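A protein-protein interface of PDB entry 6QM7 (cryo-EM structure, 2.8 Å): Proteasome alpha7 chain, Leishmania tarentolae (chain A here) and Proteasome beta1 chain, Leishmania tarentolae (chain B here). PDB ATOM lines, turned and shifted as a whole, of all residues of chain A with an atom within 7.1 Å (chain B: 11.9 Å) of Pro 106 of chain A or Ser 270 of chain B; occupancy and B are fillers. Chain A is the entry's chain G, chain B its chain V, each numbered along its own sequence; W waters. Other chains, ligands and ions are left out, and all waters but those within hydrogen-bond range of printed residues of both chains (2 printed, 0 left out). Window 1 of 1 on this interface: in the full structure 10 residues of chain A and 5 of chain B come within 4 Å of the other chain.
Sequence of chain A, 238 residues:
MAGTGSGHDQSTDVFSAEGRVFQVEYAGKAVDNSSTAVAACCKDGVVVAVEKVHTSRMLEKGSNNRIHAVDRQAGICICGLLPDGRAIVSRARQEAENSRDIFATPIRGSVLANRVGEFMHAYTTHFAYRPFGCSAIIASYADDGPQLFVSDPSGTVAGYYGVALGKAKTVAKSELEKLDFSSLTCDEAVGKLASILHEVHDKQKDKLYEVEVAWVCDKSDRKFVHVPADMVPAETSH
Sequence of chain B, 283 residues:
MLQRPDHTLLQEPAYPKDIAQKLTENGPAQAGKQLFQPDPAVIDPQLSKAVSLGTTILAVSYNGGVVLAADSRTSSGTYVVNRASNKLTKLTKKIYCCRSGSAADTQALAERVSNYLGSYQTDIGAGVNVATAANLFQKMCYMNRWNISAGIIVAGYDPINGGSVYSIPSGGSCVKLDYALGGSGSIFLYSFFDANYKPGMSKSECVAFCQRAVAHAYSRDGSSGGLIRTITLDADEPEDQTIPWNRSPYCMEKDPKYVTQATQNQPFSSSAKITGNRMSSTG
OG of Ser 270 of chain B is in hydrogen-bond range of NE of Arg 72 of chain A (2.8 Å). OG of Ser 271 of chain B lies within hydrogen-bond range of OD2 of Asp 143 of chain A, 2.6 Å away. The backbone NH (N) of Ala 272 of chain B sits at hydrogen-bond distance from the side-chain carboxylate (OD1) of Asp 143 of chain A (2.8 Å). The backbone carbonyl oxygen of Ser 270 of chain B is in hydrogen-bond range of the guanidinium group of Arg 222 of chain A, 3.2 Å away. The backbone carbonyl oxygen (O) of Ser 269 of chain B sits close to the guanidinium group (NH1) of Arg 100 of chain A, at 2.3 Å.
Pro 106 of chain A touches four residues of chain B. Of the printed residues of chain A, Ser 270 of chain B touches Arg 72 (2.8 Å), Gln 73 (3.6 Å), Pro 106 (3.7 Å), Tyr 141 (3.6 Å), Ala 142 (3.5 Å) and Arg 222 (2.4 Å). Arg 72 of chain A touches three residues of chain B. Of chain B, only Ser 270 (3.6 Å) comes within 4 Å of Gln 73 of chain A. Arg 100 of chain A touches just these residues of chain B: Phe 268 (3.3 Å) and Ser 269 (2.3 Å). Thr 105 of chain A touches one residue of chain B. No residue of chain B comes within 4 Å of Ile 107 of chain A. Of chain B, only Ser 270 comes within 4 Å of Ala 142 of chain A. Of chain B, only Ser 270 (2.4 Å) and Ser 271 (3.8 Å) come within 4 Å of Arg 222 of chain A. Of the printed residues of chain A, Ser 269 of chain B touches Arg 72, Arg 100 and Pro 106. Of the printed residues of chain B, Tyr 141 of chain A touches Ser 270 (3.6 Å). Printed residues of chain A within 4 Å of Phe 268 of chain B: Asp 71, Arg 72 and Arg 100. Arg 278 of chain B touches none of the printed residues of chain A. The nearest residue of chain B that does not touch Pro 106 of chain A is Lys 273 of chain B (6.3 Å). The nearest residue of chain A that does not touch Ser 270 of chain B is Asp 221 of chain A (4.1 Å).
Printed residues of chain B that touch a printed residue of chain A: Phe 268, Ser 269, Ser 270, Ser 271 and Ala 272. Hydrophobic or aromatic side chains of chain B within 4 Å of the printed part of chain A: Phe 268 and Ala 272. Among the printed residues, 18 pairs touch across the chains. Among the printed residues, no Asp or Glu carboxylate lies within 4 Å of a Lys or Arg side-chain nitrogen of the other chain.
Water W2 bridges NH1 of Arg 100 of chain A (2.5 Å) and N of Ser 269 of chain B (3.0 Å). Water W1 lies within hydrogen-bond range of the backbone carbonyl oxygen (O) of Phe 268 of chain B and the guanidinium group (NH1) of Arg 72 of chain A.
O of Phe 268 of chain B touches CD of Arg 72 of chain A, 3.3 Å away. Arg 72 of chain A touches Ser 269 of chain B. CE2 of Phe 268 of chain B touches NE of Arg 100 of chain A (3.3 Å). Pro 106 of chain A touches Ser 269 of chain B (CG to O, 3.9 Å). Ser 270 of chain B touches Pro 106 of chain A. Pro 106 of chain A touches Ser 271 of chain B. Tyr 141 of chain A touches Ser 270 of chain B. Ala 142 of chain A touches Ser 270 of chain B. Arg 222 of chain A touches Ser 271 of chain B.
The backbone carbonyl oxygen of Arg 72 of chain A lies within hydrogen-bond range of the backbone NH of Phe 224 of chain A (2.7 Å). The backbone carbonyl oxygen (O) of Thr 105 of chain A sits at hydrogen-bond distance from the backbone NH (N) of Arg 100 of chain A (3.4 Å). The guanidinium group (NH2) of Arg 222 of chain A is in salt-bridge range of the side-chain carboxylate (OD2) of Asp 143 of chain A, 3.6 Å away.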
ATOM      1  N   ASP A  71     -13.675 -24.309   8.452  1.00  0.00           N
ATOM      2  CA  ASP A  71     -12.285 -23.806   8.552  1.00  0.00           C
ATOM      3  C   ASP A  71     -12.362 -22.310   8.801  1.00  0.00           C
ATOM      4  O   ASP A  71     -13.478 -21.814   8.892  1.00  0.00           O
ATOM      5  CB  ASP A  71     -11.507 -24.098   7.273  1.00  0.00           C
ATOM      6  CG  ASP A  71     -10.007 -24.286   7.475  1.00  0.00           C
ATOM      7  OD1 ASP A  71      -9.493 -23.902   8.563  1.00  0.00           O
ATOM      8  OD2 ASP A  71      -9.343 -24.803   6.525  1.00  0.00           O
ATOM      9  N   ARG A  72     -11.231 -21.625   8.919  1.00  0.00           N
ATOM     10  CA  ARG A  72     -11.213 -20.141   9.024  1.00  0.00           C
ATOM     11  C   ARG A  72     -12.129 -19.563   7.939  1.00  0.00           C
ATOM     12  O   ARG A  72     -13.088 -18.858   8.293  1.00  0.00           O
ATOM     13  CB  ARG A  72      -9.792 -19.586   8.879  1.00  0.00           C
ATOM     14  CG  ARG A  72      -9.506 -18.397   9.779  1.00  0.00           C
ATOM     15  CD  ARG A  72      -8.207 -17.684   9.442  1.00  0.00           C
ATOM     16  NE  ARG A  72      -8.520 -16.402   8.828  1.00  0.00           N
ATOM     17  CZ  ARG A  72      -8.738 -15.276   9.489  1.00  0.00           C
ATOM     18  NH1 ARG A  72      -8.632 -15.222  10.808  1.00  0.00           N
ATOM     19  NH2 ARG A  72      -9.050 -14.184   8.826  1.00  0.00           N
ATOM     20  N   GLN A  73     -11.896 -19.972   6.692  1.00  0.00           N
ATOM     21  CA  GLN A  73     -12.439 -19.321   5.478  1.00  0.00           C
ATOM     22  C   GLN A  73     -13.767 -19.948   5.067  1.00  0.00           C
ATOM     23  O   GLN A  73     -14.389 -19.392   4.161  1.00  0.00           O
ATOM     24  CB  GLN A  73     -11.519 -19.409   4.258  1.00  0.00           C
ATOM     25  CG  GLN A  73     -10.335 -20.358   4.355  1.00  0.00           C
ATOM     26  CD  GLN A  73     -10.672 -21.823   4.240  1.00  0.00           C
ATOM     27  OE1 GLN A  73     -10.055 -22.662   4.888  1.00  0.00           O
ATOM     28  NE2 GLN A  73     -11.615 -22.148   3.364  1.00  0.00           N
ATOM     29  N   ALA A  74     -14.191 -21.054   5.671  1.00  0.00           N
ATOM     30  CA  ALA A  74     -15.340 -21.819   5.140  1.00  0.00           C
ATOM     31  C   ALA A  74     -16.285 -22.267   6.244  1.00  0.00           C
ATOM     32  O   ALA A  74     -15.820 -22.664   7.314  1.00  0.00           O
ATOM     33  CB  ALA A  74     -14.850 -23.010   4.357  1.00  0.00           C
ATOM     34  N   ALA A  96     -10.851 -29.967   5.407  1.00  0.00           N
ATOM     35  CA  ALA A  96     -10.276 -28.623   5.597  1.00  0.00           C
ATOM     36  C   ALA A  96      -8.952 -28.726   6.344  1.00  0.00           C
ATOM     37  O   ALA A  96      -8.046 -27.957   6.026  1.00  0.00           O
ATOM     38  CB  ALA A  96     -11.249 -27.750   6.343  1.00  0.00           C
ATOM     39  N   SER A  99      -6.223 -30.378   4.213  1.00  0.00           N
ATOM     40  CA  SER A  99      -5.670 -29.382   3.259  1.00  0.00           C
ATOM     41  C   SER A  99      -4.541 -28.605   3.942  1.00  0.00           C
ATOM     42  O   SER A  99      -3.483 -28.436   3.310  1.00  0.00           O
ATOM     43  CB  SER A  99      -6.713 -28.471   2.692  1.00  0.00           C
ATOM     44  OG  SER A  99      -6.255 -27.879   1.484  1.00  0.00           O
ATOM     45  N   ARG A 100      -4.725 -28.215   5.204  1.00  0.00           N
ATOM     46  CA  ARG A 100      -3.725 -27.423   5.965  1.00  0.00           C
ATOM     47  C   ARG A 100      -2.597 -28.339   6.453  1.00  0.00           C
ATOM     48  O   ARG A 100      -1.411 -27.957   6.314  1.00  0.00           O
ATOM     49  CB  ARG A 100      -4.424 -26.667   7.085  1.00  0.00           C
ATOM     50  CG  ARG A 100      -5.492 -25.729   6.546  1.00  0.00           C
ATOM     51  CD  ARG A 100      -6.094 -24.817   7.592  1.00  0.00           C
ATOM     52  NE  ARG A 100      -5.559 -23.490   7.379  1.00  0.00           N
ATOM     53  CZ  ARG A 100      -6.232 -22.438   6.935  1.00  0.00           C
ATOM     54  NH1 ARG A 100      -5.588 -21.302   6.780  1.00  0.00           N
ATOM     55  NH2 ARG A 100      -7.527 -22.475   6.676  1.00  0.00           N
ATOM     56  N   PHE A 103      -1.180 -30.271   2.638  1.00  0.00           N
ATOM     57  CA  PHE A 103      -0.880 -29.404   1.467  1.00  0.00           C
ATOM     58  C   PHE A 103      -0.605 -27.953   1.883  1.00  0.00           C
ATOM     59  O   PHE A 103      -0.405 -27.141   0.967  1.00  0.00           O
ATOM     60  CB  PHE A 103      -2.034 -29.487   0.466  1.00  0.00           C
ATOM     61  CG  PHE A 103      -2.262 -30.875  -0.070  1.00  0.00           C
ATOM     62  CD1 PHE A 103      -1.385 -31.426  -0.991  1.00  0.00           C
ATOM     63  CD2 PHE A 103      -3.320 -31.646   0.380  1.00  0.00           C
ATOM     64  CE1 PHE A 103      -1.563 -32.718  -1.459  1.00  0.00           C
ATOM     65  CE2 PHE A 103      -3.506 -32.934  -0.094  1.00  0.00           C
ATOM     66  CZ  PHE A 103      -2.629 -33.467  -1.015  1.00  0.00           C
ATOM     67  N   ALA A 104      -0.617 -27.624   3.182  1.00  0.00           N
ATOM     68  CA  ALA A 104      -0.220 -26.307   3.742  1.00  0.00           C
ATOM     69  C   ALA A 104      -1.029 -25.157   3.139  1.00  0.00           C
ATOM     70  O   ALA A 104      -0.489 -24.050   3.020  1.00  0.00           O
ATOM     71  CB  ALA A 104       1.251 -26.075   3.518  1.00  0.00           C
ATOM     72  N   THR A 105      -2.278 -25.400   2.783  1.00  0.00           N
ATOM     73  CA  THR A 105      -3.138 -24.400   2.110  1.00  0.00           C
ATOM     74  C   THR A 105      -4.525 -24.471   2.717  1.00  0.00           C
ATOM     75  O   THR A 105      -5.012 -25.548   3.052  1.00  0.00           O
ATOM     76  CB  THR A 105      -3.208 -24.602   0.584  1.00  0.00           C
ATOM     77  OG1 THR A 105      -3.483 -25.970   0.260  1.00  0.00           O
ATOM     78  CG2 THR A 105      -1.928 -24.181  -0.111  1.00  0.00           C
ATOM     79  N   PRO A 106      -5.202 -23.321   2.855  1.00  0.00           N
ATOM     80  CA  PRO A 106      -6.642 -23.314   3.049  1.00  0.00           C
ATOM     81  C   PRO A 106      -7.284 -24.081   1.890  1.00  0.00           C
ATOM     82  O   PRO A 106      -6.931 -23.835   0.751  1.00  0.00           O
ATOM     83  CB  PRO A 106      -7.038 -21.840   3.020  1.00  0.00           C
ATOM     84  CG  PRO A 106      -5.751 -21.098   3.299  1.00  0.00           C
ATOM     85  CD  PRO A 106      -4.626 -21.979   2.807  1.00  0.00           C
ATOM     86  N   ILE A 107      -8.168 -25.018   2.211  1.00  0.00           N
ATOM     87  CA  ILE A 107      -8.949 -25.761   1.185  1.00  0.00           C
ATOM     88  C   ILE A 107      -9.753 -24.737   0.381  1.00  0.00           C
ATOM     89  O   ILE A 107     -10.378 -23.849   0.998  1.00  0.00           O
ATOM     90  CB  ILE A 107      -9.839 -26.846   1.826  1.00  0.00           C
ATOM     91  CG1 ILE A 107     -10.328 -27.833   0.771  1.00  0.00           C
ATOM     92  CG2 ILE A 107     -10.996 -26.248   2.628  1.00  0.00           C
ATOM     93  CD1 ILE A 107     -10.823 -29.124   1.346  1.00  0.00           C
ATOM     94  N   ARG A 108      -9.716 -24.847  -0.941  1.00  0.00           N
ATOM     95  CA  ARG A 108     -10.513 -23.991  -1.848  1.00  0.00           C
ATOM     96  C   ARG A 108     -11.984 -24.368  -1.700  1.00  0.00           C
ATOM     97  O   ARG A 108     -12.267 -25.522  -1.367  1.00  0.00           O
ATOM     98  CB  ARG A 108     -10.091 -24.196  -3.302  1.00  0.00           C
ATOM     99  CG  ARG A 108      -8.632 -23.877  -3.578  1.00  0.00           C
ATOM    100  CD  ARG A 108      -8.277 -24.164  -5.023  1.00  0.00           C
ATOM    101  NE  ARG A 108      -7.269 -23.195  -5.420  1.00  0.00           N
ATOM    102  CZ  ARG A 108      -7.421 -22.241  -6.331  1.00  0.00           C
ATOM    103  NH1 ARG A 108      -8.540 -22.124  -7.034  1.00  0.00           N
ATOM    104  NH2 ARG A 108      -6.417 -21.415  -6.561  1.00  0.00           N
ATOM    105  N   GLY A 109     -12.887 -23.424  -1.928  1.00  0.00           N
ATOM    106  CA  GLY A 109     -14.336 -23.658  -1.843  1.00  0.00           C
ATOM    107  C   GLY A 109     -14.774 -24.755  -2.784  1.00  0.00           C
ATOM    108  O   GLY A 109     -15.445 -25.676  -2.316  1.00  0.00           O
ATOM    109  N   TYR A 141     -14.388 -18.421   1.397  1.00  0.00           N
ATOM    110  CA  TYR A 141     -13.646 -17.272   0.846  1.00  0.00           C
ATOM    111  C   TYR A 141     -12.164 -17.568   1.026  1.00  0.00           C
ATOM    112  O   TYR A 141     -11.440 -16.822   1.698  1.00  0.00           O
ATOM    113  CB  TYR A 141     -14.146 -15.973   1.473  1.00  0.00           C
ATOM    114  CG  TYR A 141     -13.803 -14.716   0.717  1.00  0.00           C
ATOM    115  CD1 TYR A 141     -14.449 -13.531   1.013  1.00  0.00           C
ATOM    116  CD2 TYR A 141     -12.841 -14.690  -0.285  1.00  0.00           C
ATOM    117  CE1 TYR A 141     -14.137 -12.354   0.355  1.00  0.00           C
ATOM    118  CE2 TYR A 141     -12.526 -13.523  -0.961  1.00  0.00           C
ATOM    119  CZ  TYR A 141     -13.180 -12.348  -0.640  1.00  0.00           C
ATOM    120  OH  TYR A 141     -12.877 -11.198  -1.308  1.00  0.00           O
ATOM    121  N   ALA A 142     -11.753 -18.653   0.379  1.00  0.00           N
ATOM    122  CA  ALA A 142     -10.346 -19.043   0.164  1.00  0.00           C
ATOM    123  C   ALA A 142      -9.823 -18.362  -1.109  1.00  0.00           C
ATOM    124  O   ALA A 142     -10.478 -17.416  -1.596  1.00  0.00           O
ATOM    125  CB  ALA A 142     -10.264 -20.547   0.095  1.00  0.00           C
ATOM    126  N   ASP A 143      -8.694 -18.836  -1.641  1.00  0.00           N
ATOM    127  CA  ASP A 143      -7.933 -18.163  -2.731  1.00  0.00           C
ATOM    128  C   ASP A 143      -8.723 -18.183  -4.048  1.00  0.00           C
ATOM    129  O   ASP A 143      -8.423 -17.329  -4.904  1.00  0.00           O
ATOM    130  CB  ASP A 143      -6.519 -18.749  -2.860  1.00  0.00           C
ATOM    131  CG  ASP A 143      -5.540 -18.282  -1.780  1.00  0.00           C
ATOM    132  OD1 ASP A 143      -4.640 -19.075  -1.428  1.00  0.00           O
ATOM    133  OD2 ASP A 143      -5.667 -17.126  -1.307  1.00  0.00           O
ATOM    134  N   ASP A 144      -9.732 -19.051  -4.184  1.00  0.00           N
ATOM    135  CA  ASP A 144     -10.658 -19.066  -5.353  1.00  0.00           C
ATOM    136  C   ASP A 144     -11.775 -18.019  -5.212  1.00  0.00           C
ATOM    137  O   ASP A 144     -12.732 -18.094  -6.006  1.00  0.00           O
ATOM    138  CB  ASP A 144     -11.211 -20.472  -5.616  1.00  0.00           C
ATOM    139  CG  ASP A 144     -12.095 -21.094  -4.547  1.00  0.00           C
ATOM    140  OD1 ASP A 144     -12.027 -20.653  -3.368  1.00  0.00           O
ATOM    141  OD2 ASP A 144     -12.824 -22.051  -4.903  1.00  0.00           O
ATOM    142  N   VAL A 216     -18.798 -14.766   5.468  1.00  0.00           N
ATOM    143  CA  VAL A 216     -17.325 -14.775   5.311  1.00  0.00           C
ATOM    144  C   VAL A 216     -17.050 -13.791   4.195  1.00  0.00           C
ATOM    145  O   VAL A 216     -17.403 -14.086   3.034  1.00  0.00           O
ATOM    146  CB  VAL A 216     -16.770 -16.178   5.024  1.00  0.00           C
ATOM    147  CG1 VAL A 216     -17.398 -16.825   3.800  1.00  0.00           C
ATOM    148  CG2 VAL A 216     -15.253 -16.165   4.930  1.00  0.00           C
ATOM    149  N   SER A 220     -15.099  -9.296   7.603  1.00  0.00           N
ATOM    150  CA  SER A 220     -14.866 -10.261   8.712  1.00  0.00           C
ATOM    151  C   SER A 220     -13.444 -10.835   8.679  1.00  0.00           C
ATOM    152  O   SER A 220     -13.181 -11.723   9.501  1.00  0.00           O
ATOM    153  CB  SER A 220     -15.890 -11.363   8.679  1.00  0.00           C
ATOM    154  OG  SER A 220     -15.518 -12.388   7.768  1.00  0.00           O
ATOM    155  N   ASP A 221     -12.581 -10.326   7.785  1.00  0.00           N
ATOM    156  CA  ASP A 221     -11.164 -10.737   7.555  1.00  0.00           C
ATOM    157  C   ASP A 221     -11.142 -12.084   6.820  1.00  0.00           C
ATOM    158  O   ASP A 221     -10.252 -12.901   7.088  1.00  0.00           O
ATOM    159  CB  ASP A 221     -10.353 -10.764   8.858  1.00  0.00           C
ATOM    160  CG  ASP A 221      -8.835 -10.762   8.687  1.00  0.00           C
ATOM    161  OD1 ASP A 221      -8.136 -10.931   9.717  1.00  0.00           O
ATOM    162  OD2 ASP A 221      -8.355 -10.599   7.535  1.00  0.00           O
ATOM    163  N   ARG A 222     -12.083 -12.298   5.901  1.00  0.00           N
ATOM    164  CA  ARG A 222     -12.272 -13.597   5.208  1.00  0.00           C
ATOM    165  C   ARG A 222     -12.273 -14.709   6.253  1.00  0.00           C
ATOM    166  O   ARG A 222     -11.677 -15.748   5.997  1.00  0.00           O
ATOM    167  CB  ARG A 222     -11.196 -13.772   4.134  1.00  0.00           C
ATOM    168  CG  ARG A 222     -11.371 -12.816   2.963  1.00  0.00           C
ATOM    169  CD  ARG A 222     -10.212 -12.734   1.993  1.00  0.00           C
ATOM    170  NE  ARG A 222      -9.691 -14.041   1.611  1.00  0.00           N
ATOM    171  CZ  ARG A 222      -8.880 -14.270   0.579  1.00  0.00           C
ATOM    172  NH1 ARG A 222      -8.489 -13.280  -0.210  1.00  0.00           N
ATOM    173  NH2 ARG A 222      -8.467 -15.504   0.333  1.00  0.00           N
ATOM    174  N   LYS A 223     -12.969 -14.482   7.368  1.00  0.00           N
ATOM    175  CA  LYS A 223     -13.139 -15.446   8.476  1.00  0.00           C
ATOM    176  C   LYS A 223     -14.627 -15.738   8.593  1.00  0.00           C
ATOM    177  O   LYS A 223     -15.406 -14.773   8.625  1.00  0.00           O
ATOM    178  CB  LYS A 223     -12.564 -14.875   9.770  1.00  0.00           C
ATOM    179  CG  LYS A 223     -12.088 -15.910  10.780  1.00  0.00           C
ATOM    180  CD  LYS A 223     -12.959 -16.065  12.009  1.00  0.00           C
ATOM    181  CE  LYS A 223     -12.189 -16.548  13.220  1.00  0.00           C
ATOM    182  NZ  LYS A 223     -11.431 -15.429  13.830  1.00  0.00           N
ATOM    183  N   PHE A 224     -15.007 -17.016   8.602  1.00  0.00           N
ATOM    184  CA  PHE A 224     -16.425 -17.453   8.575  1.00  0.00           C
ATOM    185  C   PHE A 224     -16.972 -17.398   9.997  1.00  0.00           C
ATOM    186  O   PHE A 224     -16.578 -18.234  10.822  1.00  0.00           O
ATOM    187  CB  PHE A 224     -16.591 -18.860   7.998  1.00  0.00           C
ATOM    188  CG  PHE A 224     -18.034 -19.268   7.894  1.00  0.00           C
ATOM    189  CD1 PHE A 224     -18.754 -18.999   6.739  1.00  0.00           C
ATOM    190  CD2 PHE A 224     -18.687 -19.849   8.970  1.00  0.00           C
ATOM    191  CE1 PHE A 224     -20.094 -19.329   6.642  1.00  0.00           C
ATOM    192  CE2 PHE A 224     -20.026 -20.189   8.873  1.00  0.00           C
ATOM    193  CZ  PHE A 224     -20.726 -19.923   7.710  1.00  0.00           C
ATOM    194  N   GLN B 266       3.914 -17.559  10.950  1.00  0.00           N
ATOM    195  CA  GLN B 266       2.836 -17.368   9.941  1.00  0.00           C
ATOM    196  C   GLN B 266       1.479 -17.475  10.612  1.00  0.00           C
ATOM    197  O   GLN B 266       1.139 -18.518  11.160  1.00  0.00           O
ATOM    198  CB  GLN B 266       2.927 -18.388   8.806  1.00  0.00           C
ATOM    199  CG  GLN B 266       2.482 -17.850   7.457  1.00  0.00           C
ATOM    200  CD  GLN B 266       2.939 -18.803   6.377  1.00  0.00           C
ATOM    201  OE1 GLN B 266       2.132 -19.420   5.683  1.00  0.00           O
ATOM    202  NE2 GLN B 266       4.248 -18.966   6.258  1.00  0.00           N
ATOM    203  N   PRO B 267       0.663 -16.402  10.580  1.00  0.00           N
ATOM    204  CA  PRO B 267      -0.628 -16.424  11.246  1.00  0.00           C
ATOM    205  C   PRO B 267      -1.554 -17.369  10.488  1.00  0.00           C
ATOM    206  O   PRO B 267      -1.356 -17.584   9.304  1.00  0.00           O
ATOM    207  CB  PRO B 267      -1.136 -14.980  11.202  1.00  0.00           C
ATOM    208  CG  PRO B 267      -0.367 -14.343  10.058  1.00  0.00           C
ATOM    209  CD  PRO B 267       0.925 -15.121   9.914  1.00  0.00           C
ATOM    210  N   PHE B 268      -2.527 -17.903  11.210  1.00  0.00           N
ATOM    211  CA  PHE B 268      -3.653 -18.696  10.671  1.00  0.00           C
ATOM    212  C   PHE B 268      -4.493 -17.787   9.770  1.00  0.00           C
ATOM    213  O   PHE B 268      -5.106 -16.816  10.287  1.00  0.00           O
ATOM    214  CB  PHE B 268      -4.456 -19.260  11.837  1.00  0.00           C
ATOM    215  CG  PHE B 268      -5.497 -20.264  11.438  1.00  0.00           C
ATOM    216  CD1 PHE B 268      -6.826 -20.078  11.793  1.00  0.00           C
ATOM    217  CD2 PHE B 268      -5.144 -21.398  10.723  1.00  0.00           C
ATOM    218  CE1 PHE B 268      -7.781 -21.014  11.449  1.00  0.00           C
ATOM    219  CE2 PHE B 268      -6.104 -22.332  10.375  1.00  0.00           C
ATOM    220  CZ  PHE B 268      -7.420 -22.138  10.739  1.00  0.00           C
ATOM    221  N   SER B 269      -4.479 -18.058   8.460  1.00  0.00           N
ATOM    222  CA  SER B 269      -5.052 -17.163   7.426  1.00  0.00           C
ATOM    223  C   SER B 269      -6.064 -17.912   6.569  1.00  0.00           C
ATOM    224  O   SER B 269      -6.146 -19.124   6.667  1.00  0.00           O
ATOM    225  CB  SER B 269      -3.977 -16.560   6.578  1.00  0.00           C
ATOM    226  OG  SER B 269      -3.562 -17.478   5.592  1.00  0.00           O
ATOM    227  N   SER B 270      -6.810 -17.169   5.763  1.00  0.00           N
ATOM    228  CA  SER B 270      -7.851 -17.689   4.848  1.00  0.00           C
ATOM    229  C   SER B 270      -7.284 -17.719   3.431  1.00  0.00           C
ATOM    230  O   SER B 270      -8.067 -17.801   2.479  1.00  0.00           O
ATOM    231  CB  SER B 270      -9.068 -16.824   4.946  1.00  0.00           C
ATOM    232  OG  SER B 270      -9.588 -16.829   6.267  1.00  0.00           O
ATOM    233  N   SER B 271      -5.959 -17.650   3.321  1.00  0.00           N
ATOM    234  CA  SER B 271      -5.206 -17.450   2.061  1.00  0.00           C
ATOM    235  C   SER B 271      -3.880 -18.201   2.163  1.00  0.00           C
ATOM    236  O   SER B 271      -3.349 -18.293   3.270  1.00  0.00           O
ATOM    237  CB  SER B 271      -4.987 -15.979   1.798  1.00  0.00           C
ATOM    238  OG  SER B 271      -4.431 -15.776   0.506  1.00  0.00           O
ATOM    239  N   ALA B 272      -3.377 -18.721   1.044  1.00  0.00           N
ATOM    240  CA  ALA B 272      -2.052 -19.375   0.936  1.00  0.00           C
ATOM    241  C   ALA B 272      -0.961 -18.314   0.757  1.00  0.00           C
ATOM    242  O   ALA B 272       0.227 -18.701   0.717  1.00  0.00           O
ATOM    243  CB  ALA B 272      -2.062 -20.346  -0.215  1.00  0.00           C
ATOM    244  N   LYS B 273      -1.343 -17.039   0.626  1.00  0.00           N
ATOM    245  CA  LYS B 273      -0.397 -15.905   0.570  1.00  0.00           C
ATOM    246  C   LYS B 273       0.397 -15.850   1.876  1.00  0.00           C
ATOM    247  O   LYS B 273      -0.213 -15.580   2.917  1.00  0.00           O
ATOM    248  CB  LYS B 273      -1.114 -14.577   0.327  1.00  0.00           C
ATOM    249  CG  LYS B 273      -0.159 -13.392   0.236  1.00  0.00           C
ATOM    250  CD  LYS B 273      -0.542 -12.335  -0.792  1.00  0.00           C
ATOM    251  CE  LYS B 273       0.585 -11.994  -1.749  1.00  0.00           C
ATOM    252  NZ  LYS B 273       1.842 -11.649  -1.041  1.00  0.00           N
ATOM    253  N   ILE B 274       1.703 -16.120   1.808  1.00  0.00           N
ATOM    254  CA  ILE B 274       2.677 -15.897   2.915  1.00  0.00           C
ATOM    255  C   ILE B 274       2.830 -14.383   3.068  1.00  0.00           C
ATOM    256  O   ILE B 274       3.231 -13.738   2.083  1.00  0.00           O
ATOM    257  CB  ILE B 274       4.025 -16.611   2.650  1.00  0.00           C
ATOM    258  CG1 ILE B 274       3.966 -18.106   2.990  1.00  0.00           C
ATOM    259  CG2 ILE B 274       5.167 -15.930   3.393  1.00  0.00           C
ATOM    260  CD1 ILE B 274       3.679 -19.017   1.821  1.00  0.00           C
ATOM    261  N   THR B 275       2.510 -13.855   4.257  1.00  0.00           N
ATOM    262  CA  THR B 275       2.615 -12.416   4.624  1.00  0.00           C
ATOM    263  C   THR B 275       3.911 -12.192   5.416  1.00  0.00           C
ATOM    264  O   THR B 275       4.888 -11.668   4.841  1.00  0.00           O
ATOM    265  CB  THR B 275       1.372 -11.955   5.400  1.00  0.00           C
ATOM    266  OG1 THR B 275       1.153 -12.879   6.468  1.00  0.00           O
ATOM    267  CG2 THR B 275       0.130 -11.863   4.536  1.00  0.00           C
ATOM    268  N   GLY B 276       3.916 -12.583   6.684  1.00  0.00           N
ATOM    269  CA  GLY B 276       5.092 -12.509   7.568  1.00  0.00           C
ATOM    270  C   GLY B 276       4.934 -13.444   8.751  1.00  0.00           C
ATOM    271  O   GLY B 276       4.000 -14.254   8.745  1.00  0.00           O
ATOM    272  N   ARG B 278       3.787 -14.150  12.566  1.00  0.00           N
ATOM    273  CA  ARG B 278       2.859 -13.686  13.618  1.00  0.00           C
ATOM    274  C   ARG B 278       3.716 -13.259  14.808  1.00  0.00           C
ATOM    275  O   ARG B 278       4.516 -14.104  15.297  1.00  0.00           O
ATOM    276  CB  ARG B 278       1.911 -14.832  13.971  1.00  0.00           C
ATOM    277  CG  ARG B 278       0.768 -14.448  14.890  1.00  0.00           C
ATOM    278  CD  ARG B 278       0.049 -15.694  15.338  1.00  0.00           C
ATOM    279  NE  ARG B 278      -0.955 -15.342  16.330  1.00  0.00           N
ATOM    280  CZ  ARG B 278      -1.482 -16.178  17.220  1.00  0.00           C
ATOM    281  NH1 ARG B 278      -2.393 -15.725  18.065  1.00  0.00           N
ATOM    282  NH2 ARG B 278      -1.126 -17.459  17.258  1.00  0.00           N
ATOM    283  N   GLY B 283      -2.897 -10.046  16.625  1.00  0.00           N
ATOM    284  CA  GLY B 283      -2.791 -10.150  15.151  1.00  0.00           C
ATOM    285  C   GLY B 283      -1.976 -11.359  14.699  1.00  0.00           C
ATOM    286  O   GLY B 283      -0.798 -11.236  14.354  1.00  0.00           O
ATOM    287  OXT GLY B 283      -2.448 -12.501  14.649  1.00  0.00           O
HETATM  288  O   HOH W   1      -5.867 -15.378  12.290  1.00  0.00           O
HETATM  289  O   HOH W   2      -3.235 -20.478   7.130  1.00  0.00           O
